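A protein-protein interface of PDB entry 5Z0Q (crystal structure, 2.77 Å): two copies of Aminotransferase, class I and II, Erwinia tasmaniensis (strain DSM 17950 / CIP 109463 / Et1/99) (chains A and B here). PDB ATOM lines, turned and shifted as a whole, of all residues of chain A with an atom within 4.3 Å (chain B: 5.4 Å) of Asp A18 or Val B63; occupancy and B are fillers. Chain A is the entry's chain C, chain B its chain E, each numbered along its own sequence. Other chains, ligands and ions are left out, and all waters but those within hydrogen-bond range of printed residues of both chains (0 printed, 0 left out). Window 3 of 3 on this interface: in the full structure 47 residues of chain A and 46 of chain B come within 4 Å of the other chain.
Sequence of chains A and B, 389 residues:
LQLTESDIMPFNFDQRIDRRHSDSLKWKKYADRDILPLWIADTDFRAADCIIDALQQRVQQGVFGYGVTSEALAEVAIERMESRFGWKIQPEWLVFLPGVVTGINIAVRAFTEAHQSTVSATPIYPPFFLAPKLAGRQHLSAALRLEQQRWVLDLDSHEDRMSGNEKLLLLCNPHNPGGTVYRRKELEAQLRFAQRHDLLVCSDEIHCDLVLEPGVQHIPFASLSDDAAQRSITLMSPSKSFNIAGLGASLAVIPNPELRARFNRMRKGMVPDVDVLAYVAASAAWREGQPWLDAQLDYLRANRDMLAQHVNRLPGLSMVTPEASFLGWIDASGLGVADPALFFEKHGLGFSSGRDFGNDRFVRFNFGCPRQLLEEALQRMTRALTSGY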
ATOM      1  N   ARG A  16     -28.850  24.947  -9.888  1.00  0.00           N
ATOM      2  CA  ARG A  16     -29.534  24.435  -8.711  1.00  0.00           C
ATOM      3  C   ARG A  16     -28.551  24.233  -7.565  1.00  0.00           C
ATOM      4  O   ARG A  16     -27.417  23.788  -7.768  1.00  0.00           O
ATOM      5  CB  ARG A  16     -30.242  23.119  -9.040  1.00  0.00           C
ATOM      6  CG  ARG A  16     -31.093  22.541  -7.909  1.00  0.00           C
ATOM      7  CD  ARG A  16     -32.313  23.408  -7.622  1.00  0.00           C
ATOM      8  NE  ARG A  16     -31.994  24.549  -6.767  1.00  0.00           N
ATOM      9  CZ  ARG A  16     -32.692  25.680  -6.738  1.00  0.00           C
ATOM     10  NH1 ARG A  16     -32.324  26.666  -5.930  1.00  0.00           N
ATOM     11  NH2 ARG A  16     -33.750  25.828  -7.522  1.00  0.00           N
ATOM     12  N   ILE A  17     -28.989  24.569  -6.353  1.00  0.00           N
ATOM     13  CA  ILE A  17     -28.183  24.417  -5.146  1.00  0.00           C
ATOM     14  C   ILE A  17     -28.808  23.323  -4.292  1.00  0.00           C
ATOM     15  O   ILE A  17     -29.983  23.413  -3.915  1.00  0.00           O
ATOM     16  CB  ILE A  17     -28.078  25.734  -4.360  1.00  0.00           C
ATOM     17  CG1 ILE A  17     -27.233  26.751  -5.130  1.00  0.00           C
ATOM     18  CG2 ILE A  17     -27.489  25.484  -2.977  1.00  0.00           C
ATOM     19  CD1 ILE A  17     -26.886  27.992  -4.330  1.00  0.00           C
ATOM     20  N   ASP A  18     -28.025  22.292  -3.991  1.00  0.00           N
ATOM     21  CA  ASP A  18     -28.454  21.195  -3.137  1.00  0.00           C
ATOM     22  C   ASP A  18     -27.874  21.357  -1.737  1.00  0.00           C
ATOM     23  O   ASP A  18     -26.906  22.090  -1.520  1.00  0.00           O
ATOM     24  CB  ASP A  18     -28.028  19.846  -3.726  1.00  0.00           C
ATOM     25  CG  ASP A  18     -28.469  19.670  -5.166  1.00  0.00           C
ATOM     26  OD1 ASP A  18     -28.844  20.675  -5.806  1.00  0.00           O
ATOM     27  OD2 ASP A  18     -28.444  18.524  -5.658  1.00  0.00           O
ATOM     28  N   ARG A  19     -28.482  20.657  -0.783  1.00  0.00           N
ATOM     29  CA  ARG A  19     -28.063  20.696   0.611  1.00  0.00           C
ATOM     30  C   ARG A  19     -27.530  19.329   1.019  1.00  0.00           C
ATOM     31  O   ARG A  19     -28.145  18.302   0.717  1.00  0.00           O
ATOM     32  CB  ARG A  19     -29.220  21.110   1.523  1.00  0.00           C
ATOM     33  CG  ARG A  19     -28.844  21.217   2.992  1.00  0.00           C
ATOM     34  CD  ARG A  19     -27.678  22.174   3.208  1.00  0.00           C
ATOM     35  NE  ARG A  19     -26.515  21.500   3.781  1.00  0.00           N
ATOM     36  CZ  ARG A  19     -25.390  22.118   4.133  1.00  0.00           C
ATOM     37  NH1 ARG A  19     -24.383  21.424   4.647  1.00  0.00           N
ATOM     38  NH2 ARG A  19     -25.274  23.429   3.974  1.00  0.00           N
ATOM     39  N   ARG A  20     -26.378  19.324   1.692  1.00  0.00           N
ATOM     40  CA  ARG A  20     -25.726  18.094   2.135  1.00  0.00           C
ATOM     41  C   ARG A  20     -25.151  18.339   3.527  1.00  0.00           C
ATOM     42  O   ARG A  20     -24.134  19.032   3.643  1.00  0.00           O
ATOM     43  CB  ARG A  20     -24.619  17.670   1.164  1.00  0.00           C
ATOM     44  CG  ARG A  20     -24.720  18.277  -0.235  1.00  0.00           C
ATOM     45  CD  ARG A  20     -24.975  17.221  -1.307  1.00  0.00           C
ATOM     46  NE  ARG A  20     -23.739  16.623  -1.807  1.00  0.00           N
ATOM     47  CZ  ARG A  20     -23.079  17.055  -2.879  1.00  0.00           C
ATOM     48  NH1 ARG A  20     -23.542  18.092  -3.563  1.00  0.00           N
ATOM     49  NH2 ARG A  20     -21.959  16.455  -3.267  1.00  0.00           N
ATOM     50  N   ASP A  44     -21.202  19.456  -7.683  1.00  0.00           N
ATOM     51  CA  ASP A  44     -22.428  19.517  -6.902  1.00  0.00           C
ATOM     52  C   ASP A  44     -23.675  19.379  -7.767  1.00  0.00           C
ATOM     53  O   ASP A  44     -24.769  19.752  -7.329  1.00  0.00           O
ATOM     54  CB  ASP A  44     -22.482  20.824  -6.108  1.00  0.00           C
ATOM     55  CG  ASP A  44     -21.324  20.965  -5.138  1.00  0.00           C
ATOM     56  OD1 ASP A  44     -20.863  19.934  -4.604  1.00  0.00           O
ATOM     57  OD2 ASP A  44     -20.875  22.108  -4.908  1.00  0.00           O
ATOM     58  N   PHE A  45     -23.534  18.846  -8.977  1.00  0.00           N
ATOM     59  CA  PHE A  45     -24.627  18.794  -9.936  1.00  0.00           C
ATOM     60  C   PHE A  45     -25.400  17.488  -9.810  1.00  0.00           C
ATOM     61  O   PHE A  45     -24.811  16.409  -9.689  1.00  0.00           O
ATOM     62  CB  PHE A  45     -24.097  18.946 -11.363  1.00  0.00           C
ATOM     63  CG  PHE A  45     -23.310  20.206 -11.587  1.00  0.00           C
ATOM     64  CD1 PHE A  45     -23.649  21.378 -10.933  1.00  0.00           C
ATOM     65  CD2 PHE A  45     -22.225  20.216 -12.448  1.00  0.00           C
ATOM     66  CE1 PHE A  45     -22.924  22.538 -11.136  1.00  0.00           C
ATOM     67  CE2 PHE A  45     -21.496  21.372 -12.656  1.00  0.00           C
ATOM     68  CZ  PHE A  45     -21.846  22.534 -11.999  1.00  0.00           C
ATOM     69  N   ARG A  46     -26.725  17.598  -9.834  1.00  0.00           N
ATOM     70  CA  ARG A  46     -27.581  16.422  -9.876  1.00  0.00           C
ATOM     71  C   ARG A  46     -27.337  15.642 -11.163  1.00  0.00           C
ATOM     72  O   ARG A  46     -27.126  16.225 -12.230  1.00  0.00           O
ATOM     73  CB  ARG A  46     -29.046  16.853  -9.768  1.00  0.00           C
ATOM     74  CG  ARG A  46     -30.077  15.778 -10.069  1.00  0.00           C
ATOM     75  CD  ARG A  46     -31.476  16.379 -10.041  1.00  0.00           C
ATOM     76  NE  ARG A  46     -32.480  15.507 -10.646  1.00  0.00           N
ATOM     77  CZ  ARG A  46     -33.271  14.688  -9.960  1.00  0.00           C
ATOM     78  NH1 ARG A  46     -33.175  14.619  -8.640  1.00  0.00           N
ATOM     79  NH2 ARG A  46     -34.156  13.933 -10.598  1.00  0.00           N
ATOM     80  N   ASN A 243     -20.608  12.907 -12.827  1.00  0.00           N
ATOM     81  CA  ASN A 243     -20.699  13.029 -11.371  1.00  0.00           C
ATOM     82  C   ASN A 243     -21.280  11.763 -10.738  1.00  0.00           C
ATOM     83  O   ASN A 243     -22.207  11.812  -9.927  1.00  0.00           O
ATOM     84  CB  ASN A 243     -21.512  14.266 -10.981  1.00  0.00           C
ATOM     85  CG  ASN A 243     -21.246  14.715  -9.560  1.00  0.00           C
ATOM     86  OD1 ASN A 243     -20.203  14.404  -8.982  1.00  0.00           O
ATOM     87  ND2 ASN A 243     -22.187  15.459  -8.989  1.00  0.00           N
ATOM     88  N   ARG B  58     -32.371   7.346  -1.905  1.00  0.00           N
ATOM     89  CA  ARG B  58     -31.015   7.806  -2.181  1.00  0.00           C
ATOM     90  C   ARG B  58     -30.833   8.131  -3.660  1.00  0.00           C
ATOM     91  O   ARG B  58     -30.098   9.061  -4.012  1.00  0.00           O
ATOM     92  CB  ARG B  58     -30.002   6.752  -1.730  1.00  0.00           C
ATOM     93  CG  ARG B  58     -28.549   7.120  -1.989  1.00  0.00           C
ATOM     94  CD  ARG B  58     -28.147   8.368  -1.226  1.00  0.00           C
ATOM     95  NE  ARG B  58     -26.790   8.793  -1.551  1.00  0.00           N
ATOM     96  CZ  ARG B  58     -26.492   9.662  -2.511  1.00  0.00           C
ATOM     97  NH1 ARG B  58     -25.230   9.996  -2.739  1.00  0.00           N
ATOM     98  NH2 ARG B  58     -27.460  10.200  -3.242  1.00  0.00           N
ATOM     99  N   GLN B  61     -32.228  11.589  -4.610  1.00  0.00           N
ATOM    100  CA  GLN B  61     -31.461  12.755  -4.183  1.00  0.00           C
ATOM    101  C   GLN B  61     -30.707  13.378  -5.350  1.00  0.00           C
ATOM    102  O   GLN B  61     -30.541  14.602  -5.399  1.00  0.00           O
ATOM    103  CB  GLN B  61     -30.497  12.375  -3.061  1.00  0.00           C
ATOM    104  CG  GLN B  61     -31.183  12.016  -1.753  1.00  0.00           C
ATOM    105  CD  GLN B  61     -30.200  11.768  -0.626  1.00  0.00           C
ATOM    106  OE1 GLN B  61     -28.990  11.926  -0.795  1.00  0.00           O
ATOM    107  NE2 GLN B  61     -30.717  11.377   0.535  1.00  0.00           N
ATOM    108  N   GLY B  62     -30.243  12.558  -6.296  1.00  0.00           N
ATOM    109  CA  GLY B  62     -29.708  13.022  -7.553  1.00  0.00           C
ATOM    110  C   GLY B  62     -28.193  13.048  -7.641  1.00  0.00           C
ATOM    111  O   GLY B  62     -27.645  12.799  -8.720  1.00  0.00           O
ATOM    112  N   VAL B  63     -27.507  13.344  -6.540  1.00  0.00           N
ATOM    113  CA  VAL B  63     -26.059  13.534  -6.542  1.00  0.00           C
ATOM    114  C   VAL B  63     -25.385  12.236  -6.119  1.00  0.00           C
ATOM    115  O   VAL B  63     -25.718  11.664  -5.073  1.00  0.00           O
ATOM    116  CB  VAL B  63     -25.650  14.693  -5.617  1.00  0.00           C
ATOM    117  CG1 VAL B  63     -24.154  14.940  -5.711  1.00  0.00           C
ATOM    118  CG2 VAL B  63     -26.427  15.950  -5.975  1.00  0.00           C
ATOM    119  N   PHE B  64     -24.433  11.773  -6.929  1.00  0.00           N
ATOM    120  CA  PHE B  64     -23.737  10.521  -6.653  1.00  0.00           C
ATOM    121  C   PHE B  64     -22.229  10.731  -6.591  1.00  0.00           C
ATOM    122  O   PHE B  64     -21.465   9.968  -7.190  1.00  0.00           O
ATOM    123  CB  PHE B  64     -24.087   9.472  -7.711  1.00  0.00           C
ATOM    124  CG  PHE B  64     -25.561   9.202  -7.829  1.00  0.00           C
ATOM    125  CD1 PHE B  64     -26.196   8.349  -6.942  1.00  0.00           C
ATOM    126  CD2 PHE B  64     -26.311   9.804  -8.825  1.00  0.00           C
ATOM    127  CE1 PHE B  64     -27.551   8.102  -7.044  1.00  0.00           C
ATOM    128  CE2 PHE B  64     -27.667   9.561  -8.934  1.00  0.00           C
ATOM    129  CZ  PHE B  64     -28.288   8.708  -8.042  1.00  0.00           C
ATOM    130  N   GLY B  65     -21.794  11.761  -5.872  1.00  0.00           N
ATOM    131  CA  GLY B  65     -20.384  12.016  -5.680  1.00  0.00           C
ATOM    132  C   GLY B  65     -19.781  11.099  -4.633  1.00  0.00           C
ATOM    133  O   GLY B  65     -20.404  10.151  -4.152  1.00  0.00           O
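O of Asn A243 sits close to O of Phe B64, 3.4 Å away.
OD1 of Asp A44 is in salt-bridge range of NH1 of Arg A20, 3.4 Å away.
The backbone carbonyl oxygen of Phe A45 sits at hydrogen-bond distance from the side-chain amide nitrogen of Asn A243, 2.9 Å away.
The backbone carbonyl oxygen of Val B63 sits at hydrogen-bond distance from the guanidinium group of Arg B58, at 2.9 Å.
Val B63 touches Asp A18.
Val B63 touches Arg A20.
Gly B62 touches Arg A46 (CA to CG, 3.7 Å).
CG1 of Val B63 touches ND2 of Asn A243 (3.9 Å).
Of chain B, only Val B63 comes within 4 Å of Asp A18.
Val B63 touches three residues of chain A.
Of the printed residues of chain B, Arg A46 touches Gly B62.
Of the printed residues of chain B, Arg A20 touches Val B63 (3.6 Å).
Gln B61 touches none of the printed residues of chain A.
The nearest residue of chain B that does not touch Asp A18 is Gln B61 (4.5 Å).
The nearest printed residue of chain A that does not touch Val B63 is Phe A45 (4.1 Å).
Printed residues of chain B that touch a printed residue of chain A: Gly B62, Val B63 and Phe B64.
Hydrophobic or aromatic side chains of chain B that line the printed part of chain A: Val B63 and Phe B64.
Of the 9 printed residues of chain A, 4 touch a printed residue of chain B.
Printed residues of chain A that touch a printed residue of chain B: Asp A18, Arg A20, Arg A46 and Asn A243.
Among the printed residues, no Asp or Glu carboxylate lies within 4 Å of a Lys or Arg side-chain nitrogen of the other chain.
No position is printed for both chains.
Of the 5 pairs that touch across the chains among the printed residues, none has its exchanged pair printed and touching as well.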
